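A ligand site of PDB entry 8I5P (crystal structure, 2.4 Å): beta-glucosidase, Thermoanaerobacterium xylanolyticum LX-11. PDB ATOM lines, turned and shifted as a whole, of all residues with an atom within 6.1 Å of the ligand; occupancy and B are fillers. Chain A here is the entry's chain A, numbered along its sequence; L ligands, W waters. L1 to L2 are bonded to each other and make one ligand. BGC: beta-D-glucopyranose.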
ATOM      1  N   TYR A  47      25.968  -2.406   0.403  1.00  0.00           N
ATOM      2  CA  TYR A  47      25.529  -3.754   0.012  1.00  0.00           C
ATOM      3  C   TYR A  47      26.555  -4.415  -0.934  1.00  0.00           C
ATOM      4  O   TYR A  47      27.379  -3.722  -1.517  1.00  0.00           O
ATOM      5  CB  TYR A  47      24.094  -3.774  -0.574  1.00  0.00           C
ATOM      6  CG  TYR A  47      23.855  -2.955  -1.848  1.00  0.00           C
ATOM      7  CD1 TYR A  47      23.519  -1.585  -1.782  1.00  0.00           C
ATOM      8  CD2 TYR A  47      23.919  -3.554  -3.122  1.00  0.00           C
ATOM      9  CE1 TYR A  47      23.282  -0.849  -2.932  1.00  0.00           C
ATOM     10  CE2 TYR A  47      23.682  -2.810  -4.283  1.00  0.00           C
ATOM     11  CZ  TYR A  47      23.371  -1.472  -4.190  1.00  0.00           C
ATOM     12  OH  TYR A  47      23.135  -0.722  -5.339  1.00  0.00           O
ATOM     13  N   GLU A 426      20.121  -5.431 -17.677  1.00  0.00           N
ATOM     14  CA  GLU A 426      20.438  -4.117 -17.139  1.00  0.00           C
ATOM     15  C   GLU A 426      21.903  -4.126 -16.691  1.00  0.00           C
ATOM     16  O   GLU A 426      22.680  -3.268 -17.079  1.00  0.00           O
ATOM     17  CB  GLU A 426      19.501  -3.787 -15.960  1.00  0.00           C
ATOM     18  CG  GLU A 426      19.856  -2.503 -15.203  1.00  0.00           C
ATOM     19  CD  GLU A 426      18.883  -2.151 -14.083  1.00  0.00           C
ATOM     20  OE1 GLU A 426      17.808  -2.779 -13.968  1.00  0.00           O
ATOM     21  OE2 GLU A 426      19.208  -1.230 -13.314  1.00  0.00           O
ATOM     22  N   ASP A 429      24.628  -7.142 -11.340  1.00  0.00           N
ATOM     23  CA  ASP A 429      24.177  -6.837  -9.980  1.00  0.00           C
ATOM     24  C   ASP A 429      22.663  -6.648  -9.863  1.00  0.00           C
ATOM     25  O   ASP A 429      22.054  -7.070  -8.889  1.00  0.00           O
ATOM     26  CB  ASP A 429      24.840  -5.547  -9.473  1.00  0.00           C
ATOM     27  CG  ASP A 429      26.333  -5.696  -9.269  1.00  0.00           C
ATOM     28  OD1 ASP A 429      26.747  -6.506  -8.396  1.00  0.00           O
ATOM     29  OD2 ASP A 429      27.093  -4.985  -9.955  1.00  0.00           O
ATOM     30  N   TYR A 430      22.077  -5.985 -10.868  1.00  0.00           N
ATOM     31  CA  TYR A 430      20.639  -5.779 -10.940  1.00  0.00           C
ATOM     32  C   TYR A 430      20.163  -6.644 -12.108  1.00  0.00           C
ATOM     33  O   TYR A 430      19.992  -6.174 -13.239  1.00  0.00           O
ATOM     34  CB  TYR A 430      20.292  -4.302 -11.164  1.00  0.00           C
ATOM     35  CG  TYR A 430      21.029  -3.282 -10.308  1.00  0.00           C
ATOM     36  CD1 TYR A 430      21.398  -3.561  -8.983  1.00  0.00           C
ATOM     37  CD2 TYR A 430      21.324  -2.015 -10.810  1.00  0.00           C
ATOM     38  CE1 TYR A 430      22.055  -2.610  -8.212  1.00  0.00           C
ATOM     39  CE2 TYR A 430      21.979  -1.069 -10.051  1.00  0.00           C
ATOM     40  CZ  TYR A 430      22.345  -1.360  -8.752  1.00  0.00           C
ATOM     41  OH  TYR A 430      22.994  -0.399  -7.999  1.00  0.00           O
ATOM     42  N   TYR A 432      18.159  -8.030 -14.241  1.00  0.00           N
ATOM     43  CA  TYR A 432      16.858  -7.869 -14.887  1.00  0.00           C
ATOM     44  C   TYR A 432      17.030  -7.707 -16.402  1.00  0.00           C
ATOM     45  O   TYR A 432      17.777  -6.835 -16.856  1.00  0.00           O
ATOM     46  CB  TYR A 432      16.115  -6.671 -14.312  1.00  0.00           C
ATOM     47  CG  TYR A 432      16.112  -6.622 -12.803  1.00  0.00           C
ATOM     48  CD1 TYR A 432      15.592  -7.684 -12.048  1.00  0.00           C
ATOM     49  CD2 TYR A 432      16.624  -5.524 -12.128  1.00  0.00           C
ATOM     50  CE1 TYR A 432      15.603  -7.644 -10.662  1.00  0.00           C
ATOM     51  CE2 TYR A 432      16.635  -5.470 -10.740  1.00  0.00           C
ATOM     52  CZ  TYR A 432      16.123  -6.528 -10.019  1.00  0.00           C
ATOM     53  OH  TYR A 432      16.144  -6.451  -8.651  1.00  0.00           O
ATOM     54  N   THR A 435      15.419  -4.000 -18.856  1.00  0.00           N
ATOM     55  CA  THR A 435      14.837  -2.968 -17.999  1.00  0.00           C
ATOM     56  C   THR A 435      14.498  -1.736 -18.839  1.00  0.00           C
ATOM     57  O   THR A 435      15.393  -1.088 -19.410  1.00  0.00           O
ATOM     58  CB  THR A 435      15.758  -2.592 -16.841  1.00  0.00           C
ATOM     59  OG1 THR A 435      15.992  -3.761 -16.049  1.00  0.00           O
ATOM     60  CG2 THR A 435      15.120  -1.547 -15.959  1.00  0.00           C
ATOM     61  N   ASP A 437      13.320   1.432 -18.568  1.00  0.00           N
ATOM     62  CA  ASP A 437      13.806   2.786 -18.327  1.00  0.00           C
ATOM     63  C   ASP A 437      15.297   2.960 -18.652  1.00  0.00           C
ATOM     64  O   ASP A 437      15.732   4.067 -18.988  1.00  0.00           O
ATOM     65  CB  ASP A 437      13.461   3.248 -16.910  1.00  0.00           C
ATOM     66  CG  ASP A 437      14.415   2.730 -15.842  1.00  0.00           C
ATOM     67  OD1 ASP A 437      14.297   1.568 -15.434  1.00  0.00           O
ATOM     68  OD2 ASP A 437      15.241   3.537 -15.362  1.00  0.00           O
ATOM     69  N   VAL A 438      16.047   1.868 -18.573  1.00  0.00           N
ATOM     70  CA  VAL A 438      17.465   1.825 -18.924  1.00  0.00           C
ATOM     71  C   VAL A 438      17.642   1.674 -20.439  1.00  0.00           C
ATOM     72  O   VAL A 438      18.487   2.317 -21.034  1.00  0.00           O
ATOM     73  CB  VAL A 438      18.158   0.660 -18.181  1.00  0.00           C
ATOM     74  CG1 VAL A 438      19.638   0.539 -18.543  1.00  0.00           C
ATOM     75  CG2 VAL A 438      17.997   0.820 -16.679  1.00  0.00           C
ATOM     76  N   HIS A 492       8.619  -2.965 -15.593  1.00  0.00           N
ATOM     77  CA  HIS A 492       9.980  -2.526 -15.352  1.00  0.00           C
ATOM     78  C   HIS A 492      10.979  -3.318 -16.180  1.00  0.00           C
ATOM     79  O   HIS A 492      11.943  -2.762 -16.703  1.00  0.00           O
ATOM     80  CB  HIS A 492      10.297  -2.684 -13.873  1.00  0.00           C
ATOM     81  CG  HIS A 492      11.697  -2.295 -13.496  1.00  0.00           C
ATOM     82  ND1 HIS A 492      12.714  -3.218 -13.369  1.00  0.00           N
ATOM     83  CD2 HIS A 492      12.245  -1.087 -13.219  1.00  0.00           C
ATOM     84  CE1 HIS A 492      13.825  -2.600 -13.032  1.00  0.00           C
ATOM     85  NE2 HIS A 492      13.574  -1.299 -12.929  1.00  0.00           N
ATOM     86  N   TYR A 508      12.022  -7.151 -10.728  1.00  0.00           N
ATOM     87  CA  TYR A 508      12.354  -6.019  -9.859  1.00  0.00           C
ATOM     88  C   TYR A 508      11.236  -5.749  -8.834  1.00  0.00           C
ATOM     89  O   TYR A 508      10.089  -5.496  -9.204  1.00  0.00           O
ATOM     90  CB  TYR A 508      12.577  -4.800 -10.721  1.00  0.00           C
ATOM     91  CG  TYR A 508      12.709  -3.457 -10.026  1.00  0.00           C
ATOM     92  CD1 TYR A 508      13.943  -3.042  -9.525  1.00  0.00           C
ATOM     93  CD2 TYR A 508      11.623  -2.597  -9.937  1.00  0.00           C
ATOM     94  CE1 TYR A 508      14.065  -1.803  -8.914  1.00  0.00           C
ATOM     95  CE2 TYR A 508      11.750  -1.351  -9.331  1.00  0.00           C
ATOM     96  CZ  TYR A 508      12.979  -0.957  -8.827  1.00  0.00           C
ATOM     97  OH  TYR A 508      13.118   0.267  -8.220  1.00  0.00           O
ATOM     98  N   ASP A 509      11.595  -5.789  -7.554  1.00  0.00           N
ATOM     99  CA  ASP A 509      10.657  -5.623  -6.433  1.00  0.00           C
ATOM    100  C   ASP A 509      11.081  -4.572  -5.414  1.00  0.00           C
ATOM    101  O   ASP A 509      10.408  -4.369  -4.419  1.00  0.00           O
ATOM    102  CB  ASP A 509      10.421  -6.969  -5.723  1.00  0.00           C
ATOM    103  CG  ASP A 509      11.722  -7.652  -5.270  1.00  0.00           C
ATOM    104  OD1 ASP A 509      12.755  -6.959  -5.098  1.00  0.00           O
ATOM    105  OD2 ASP A 509      11.722  -8.885  -5.085  1.00  0.00           O
ATOM    106  N   TRP A 510      12.182  -3.874  -5.666  1.00  0.00           N
ATOM    107  CA  TRP A 510      12.689  -2.901  -4.730  1.00  0.00           C
ATOM    108  C   TRP A 510      11.785  -1.664  -4.599  1.00  0.00           C
ATOM    109  O   TRP A 510      11.717  -1.035  -3.549  1.00  0.00           O
ATOM    110  CB  TRP A 510      14.099  -2.472  -5.116  1.00  0.00           C
ATOM    111  CG  TRP A 510      14.757  -1.834  -3.975  1.00  0.00           C
ATOM    112  CD1 TRP A 510      15.070  -0.511  -3.825  1.00  0.00           C
ATOM    113  CD2 TRP A 510      15.095  -2.486  -2.759  1.00  0.00           C
ATOM    114  NE1 TRP A 510      15.629  -0.309  -2.576  1.00  0.00           N
ATOM    115  CE2 TRP A 510      15.646  -1.506  -1.902  1.00  0.00           C
ATOM    116  CE3 TRP A 510      14.993  -3.809  -2.302  1.00  0.00           C
ATOM    117  CZ2 TRP A 510      16.108  -1.810  -0.623  1.00  0.00           C
ATOM    118  CZ3 TRP A 510      15.443  -4.105  -1.025  1.00  0.00           C
ATOM    119  CH2 TRP A 510      15.997  -3.116  -0.197  1.00  0.00           C
ATOM    120  N   TRP A 516       4.934   3.955 -11.653  1.00  0.00           N
ATOM    121  CA  TRP A 516       5.933   4.820 -12.281  1.00  0.00           C
ATOM    122  C   TRP A 516       5.264   5.682 -13.351  1.00  0.00           C
ATOM    123  O   TRP A 516       4.334   5.245 -14.035  1.00  0.00           O
ATOM    124  CB  TRP A 516       7.120   4.034 -12.846  1.00  0.00           C
ATOM    125  CG  TRP A 516       8.113   3.545 -11.796  1.00  0.00           C
ATOM    126  CD1 TRP A 516       7.849   3.296 -10.465  1.00  0.00           C
ATOM    127  CD2 TRP A 516       9.496   3.224 -11.985  1.00  0.00           C
ATOM    128  NE1 TRP A 516       8.979   2.847  -9.832  1.00  0.00           N
ATOM    129  CE2 TRP A 516      10.007   2.801 -10.737  1.00  0.00           C
ATOM    130  CE3 TRP A 516      10.355   3.257 -13.094  1.00  0.00           C
ATOM    131  CZ2 TRP A 516      11.334   2.408 -10.559  1.00  0.00           C
ATOM    132  CZ3 TRP A 516      11.683   2.878 -12.915  1.00  0.00           C
ATOM    133  CH2 TRP A 516      12.166   2.455 -11.655  1.00  0.00           C
ATOM    134  N   THR A 576      12.441   6.424 -12.741  1.00  0.00           N
ATOM    135  CA  THR A 576      13.872   6.071 -12.827  1.00  0.00           C
ATOM    136  C   THR A 576      14.735   6.554 -11.673  1.00  0.00           C
ATOM    137  O   THR A 576      15.501   5.777 -11.114  1.00  0.00           O
ATOM    138  CB  THR A 576      14.454   6.659 -14.125  1.00  0.00           C
ATOM    139  OG1 THR A 576      13.845   6.012 -15.243  1.00  0.00           O
ATOM    140  CG2 THR A 576      15.958   6.470 -14.232  1.00  0.00           C
ATOM    141  N   THR A 579      14.778   7.335  -5.651  1.00  0.00           N
ATOM    142  CA  THR A 579      15.100   7.926  -4.349  1.00  0.00           C
ATOM    143  C   THR A 579      15.361   9.434  -4.400  1.00  0.00           C
ATOM    144  O   THR A 579      15.321  10.100  -3.370  1.00  0.00           O
ATOM    145  CB  THR A 579      16.280   7.189  -3.685  1.00  0.00           C
ATOM    146  OG1 THR A 579      17.426   7.255  -4.522  1.00  0.00           O
ATOM    147  CG2 THR A 579      15.925   5.743  -3.446  1.00  0.00           C
ATOM    148  N   GLN A 712      21.579   9.709  -5.667  1.00  0.00           N
ATOM    149  CA  GLN A 712      21.415   9.728  -7.124  1.00  0.00           C
ATOM    150  C   GLN A 712      21.720  11.092  -7.733  1.00  0.00           C
ATOM    151  O   GLN A 712      22.333  11.174  -8.804  1.00  0.00           O
ATOM    152  CB  GLN A 712      19.997   9.296  -7.503  1.00  0.00           C
ATOM    153  CG  GLN A 712      19.683   7.846  -7.166  1.00  0.00           C
ATOM    154  CD  GLN A 712      18.319   7.421  -7.686  1.00  0.00           C
ATOM    155  OE1 GLN A 712      17.388   8.212  -7.717  1.00  0.00           O
ATOM    156  NE2 GLN A 712      18.201   6.171  -8.113  1.00  0.00           N
ATOM    157  N   GLU A 715      25.393  11.632  -8.148  1.00  0.00           N
ATOM    158  CA  GLU A 715      26.030  10.715  -9.095  1.00  0.00           C
ATOM    159  C   GLU A 715      26.087  11.295 -10.513  1.00  0.00           C
ATOM    160  O   GLU A 715      25.178  12.013 -10.951  1.00  0.00           O
ATOM    161  CB  GLU A 715      25.272   9.386  -9.128  1.00  0.00           C
ATOM    162  CG  GLU A 715      25.504   8.530  -7.907  1.00  0.00           C
ATOM    163  CD  GLU A 715      24.714   7.235  -7.921  1.00  0.00           C
ATOM    164  OE1 GLU A 715      23.558   7.215  -8.408  1.00  0.00           O
ATOM    165  OE2 GLU A 715      25.260   6.235  -7.445  1.00  0.00           O
ATOM    166  N   TRP A 717      25.658   9.714 -13.994  1.00  0.00           N
ATOM    167  CA  TRP A 717      25.200   8.496 -14.691  1.00  0.00           C
ATOM    168  C   TRP A 717      25.786   8.485 -16.099  1.00  0.00           C
ATOM    169  O   TRP A 717      25.461   9.345 -16.912  1.00  0.00           O
ATOM    170  CB  TRP A 717      23.674   8.401 -14.717  1.00  0.00           C
ATOM    171  CG  TRP A 717      23.051   8.028 -13.373  1.00  0.00           C
ATOM    172  CD1 TRP A 717      23.654   8.067 -12.142  1.00  0.00           C
ATOM    173  CD2 TRP A 717      21.693   7.627 -13.139  1.00  0.00           C
ATOM    174  NE1 TRP A 717      22.761   7.692 -11.163  1.00  0.00           N
ATOM    175  CE2 TRP A 717      21.547   7.434 -11.746  1.00  0.00           C
ATOM    176  CE3 TRP A 717      20.579   7.434 -13.967  1.00  0.00           C
ATOM    177  CZ2 TRP A 717      20.346   7.025 -11.168  1.00  0.00           C
ATOM    178  CZ3 TRP A 717      19.378   7.025 -13.389  1.00  0.00           C
ATOM    179  CH2 TRP A 717      19.271   6.826 -12.005  1.00  0.00           C
ATOM    180  N   GLU A 762      27.103   2.106 -14.248  1.00  0.00           N
ATOM    181  CA  GLU A 762      25.971   3.041 -14.257  1.00  0.00           C
ATOM    182  C   GLU A 762      26.463   4.404 -13.817  1.00  0.00           C
ATOM    183  O   GLU A 762      26.230   5.406 -14.495  1.00  0.00           O
ATOM    184  CB  GLU A 762      24.861   2.571 -13.295  1.00  0.00           C
ATOM    185  CG  GLU A 762      23.833   3.638 -12.870  1.00  0.00           C
ATOM    186  CD  GLU A 762      22.723   3.847 -13.872  1.00  0.00           C
ATOM    187  OE1 GLU A 762      22.973   4.373 -14.984  1.00  0.00           O
ATOM    188  OE2 GLU A 762      21.562   3.498 -13.553  1.00  0.00           O
ATOM    189  N   ARG A 771      29.051   2.666  -8.929  1.00  0.00           N
ATOM    190  CA  ARG A 771      27.923   1.782  -8.659  1.00  0.00           C
ATOM    191  C   ARG A 771      27.552   1.003  -9.925  1.00  0.00           C
ATOM    192  O   ARG A 771      27.395   1.594 -10.988  1.00  0.00           O
ATOM    193  CB  ARG A 771      26.741   2.587  -8.151  1.00  0.00           C
ATOM    194  CG  ARG A 771      25.508   1.778  -7.833  1.00  0.00           C
ATOM    195  CD  ARG A 771      24.496   2.639  -7.120  1.00  0.00           C
ATOM    196  NE  ARG A 771      23.946   3.692  -7.978  1.00  0.00           N
ATOM    197  CZ  ARG A 771      22.974   3.533  -8.877  1.00  0.00           C
ATOM    198  NH1 ARG A 771      22.410   2.340  -9.097  1.00  0.00           N
ATOM    199  NH2 ARG A 771      22.554   4.581  -9.569  1.00  0.00           N
ATOM    200  N   TYR A 775      27.220  -2.176 -17.159  1.00  0.00           N
ATOM    201  CA  TYR A 775      25.867  -1.604 -17.212  1.00  0.00           C
ATOM    202  C   TYR A 775      25.398  -1.298 -18.647  1.00  0.00           C
ATOM    203  O   TYR A 775      26.180  -0.844 -19.477  1.00  0.00           O
ATOM    204  CB  TYR A 775      25.805  -0.332 -16.338  1.00  0.00           C
ATOM    205  CG  TYR A 775      24.422  -0.046 -15.788  1.00  0.00           C
ATOM    206  CD1 TYR A 775      23.884  -0.823 -14.755  1.00  0.00           C
ATOM    207  CD2 TYR A 775      23.640   0.975 -16.292  1.00  0.00           C
ATOM    208  CE1 TYR A 775      22.605  -0.590 -14.264  1.00  0.00           C
ATOM    209  CE2 TYR A 775      22.355   1.223 -15.808  1.00  0.00           C
ATOM    210  CZ  TYR A 775      21.842   0.441 -14.798  1.00  0.00           C
ATOM    211  OH  TYR A 775      20.561   0.691 -14.331  1.00  0.00           O
ATOM    212  N   ARG A 777      23.137   1.004 -19.808  1.00  0.00           N
ATOM    213  CA  ARG A 777      22.870   2.419 -20.138  1.00  0.00           C
ATOM    214  C   ARG A 777      23.927   3.175 -20.966  1.00  0.00           C
ATOM    215  O   ARG A 777      23.549   3.911 -21.880  1.00  0.00           O
ATOM    216  CB  ARG A 777      22.507   3.246 -18.893  1.00  0.00           C
ATOM    217  CG  ARG A 777      21.516   4.364 -19.198  1.00  0.00           C
ATOM    218  CD  ARG A 777      21.362   5.362 -18.055  1.00  0.00           C
ATOM    219  NE  ARG A 777      20.930   4.733 -16.804  1.00  0.00           N
ATOM    220  CZ  ARG A 777      19.669   4.555 -16.402  1.00  0.00           C
ATOM    221  NH1 ARG A 777      18.636   4.956 -17.142  1.00  0.00           N
ATOM    222  NH2 ARG A 777      19.431   3.967 -15.240  1.00  0.00           N
HETATM  223  C2  BGC L   1      19.667   0.458  -6.253  1.00  0.00           C
HETATM  224  C3  BGC L   1      18.811   0.811  -7.469  1.00  0.00           C
HETATM  225  C4  BGC L   1      18.490  -0.438  -8.293  1.00  0.00           C
HETATM  226  C5  BGC L   1      18.006  -1.598  -7.420  1.00  0.00           C
HETATM  227  C6  BGC L   1      17.825  -2.879  -8.238  1.00  0.00           C
HETATM  228  C1  BGC L   1      19.014  -0.689  -5.483  1.00  0.00           C
HETATM  229  O1  BGC L   1      19.777  -1.029  -4.318  1.00  0.00           O
HETATM  230  O2  BGC L   1      19.841   1.618  -5.442  1.00  0.00           O
HETATM  231  O3  BGC L   1      19.502   1.802  -8.250  1.00  0.00           O
HETATM  232  O4  BGC L   1      17.421  -0.135  -9.187  1.00  0.00           O
HETATM  233  O5  BGC L   1      18.933  -1.824  -6.348  1.00  0.00           O
HETATM  234  O6  BGC L   1      17.036  -3.851  -7.555  1.00  0.00           O
HETATM  235  C2  BGC L   2      16.533   0.002 -11.370  1.00  0.00           C
HETATM  236  C3  BGC L   2      16.507   0.820 -12.660  1.00  0.00           C
HETATM  237  C4  BGC L   2      17.061   2.223 -12.488  1.00  0.00           C
HETATM  238  C5  BGC L   2      18.407   2.181 -11.761  1.00  0.00           C
HETATM  239  C6  BGC L   2      19.071   3.546 -11.585  1.00  0.00           C
HETATM  240  C1  BGC L   2      17.780   0.254 -10.507  1.00  0.00           C
HETATM  241  O2  BGC L   2      16.462  -1.386 -11.692  1.00  0.00           O
HETATM  242  O3  BGC L   2      15.158   0.878 -13.113  1.00  0.00           O
HETATM  243  O4  BGC L   2      17.191   2.818 -13.782  1.00  0.00           O
HETATM  244  O5  BGC L   2      18.189   1.630 -10.478  1.00  0.00           O
HETATM  245  O6  BGC L   2      20.414   3.346 -11.130  1.00  0.00           O
HETATM  246  O   HOH W   1      22.363   1.834  -4.557  1.00  0.00           O
HETATM  247  O   HOH W   2      20.148   4.200  -7.159  1.00  0.00           O
HETATM  248  O   HOH W   3      18.961  -2.863  -2.396  1.00  0.00           O
HETATM  249  O   HOH W   4      19.527  -0.087  -1.459  1.00  0.00           O
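The side-chain carboxylate (OD1) of Asp 437 is in hydrogen-bond range of an oxygen (O3) of BGC L2, at 2.6 Å. O6 of BGC L2 sits at hydrogen-bond distance from OE2 of Glu 762 (2.7 Å). A ring nitrogen (NE2) of His 492 is in hydrogen-bond range of an oxygen (O3) of BGC L2 (2.7 Å). An oxygen (O4) of BGC L2 sits at hydrogen-bond distance from the guanidinium group (NH2) of Arg 777 (2.9 Å). O6 of BGC L2 lies within hydrogen-bond range of NH2 of Arg 771. An oxygen (O6) of BGC L1 lies within hydrogen-bond range of the side-chain hydroxyl (OH) of Tyr 432 (3.0 Å). The side-chain carboxylate (OE1) of Glu 426 lies within hydrogen-bond range of an oxygen (O2) of BGC L2 (3.0 Å).
Residues that only touch the ligand: Tyr 47, Tyr 430, Thr 435, Val 438, Tyr 508, Trp 516, Thr 576, Trp 717 and Tyr 775. Along chain A the residues within 4 Å of the ligand span positions 47 to 777.
Water W1 lies within hydrogen-bond range of O2 of BGC L1 (2.7 Å) and OH of Tyr 47 (2.8 Å). Water W2 lies within hydrogen-bond range of O3 of BGC L1 (2.7 Å), NE2 of Gln 712 (2.9 Å) and NH2 of Arg 771 (3.4 Å).
OE2 of Glu 762 lies within salt-bridge range of NH2 of Arg 777, 2.8 Å away. The backbone carbonyl oxygen (O) of Arg 771 is in hydrogen-bond range of the backbone NH (N) of Glu 762 (3.3 Å). OH of Tyr 775 sits at hydrogen-bond distance from OE2 of Glu 762 (3.1 Å). NH1 of Arg 771 lies within hydrogen-bond range of OH of Tyr 430 (3.0 Å). NE of Arg 771 lies within salt-bridge range of OE2 of Glu 715 (2.9 Å). The backbone carbonyl oxygen (O) of Tyr 432 lies within hydrogen-bond range of the backbone NH (N) of Glu 426 (2.9 Å). OE1 of Glu 426 is in hydrogen-bond range of OG1 of Thr 435, at 2.9 Å. The side-chain hydroxyl of Tyr 47 is in hydrogen-bond range of the side-chain hydroxyl of Tyr 430, 2.7 Å away.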
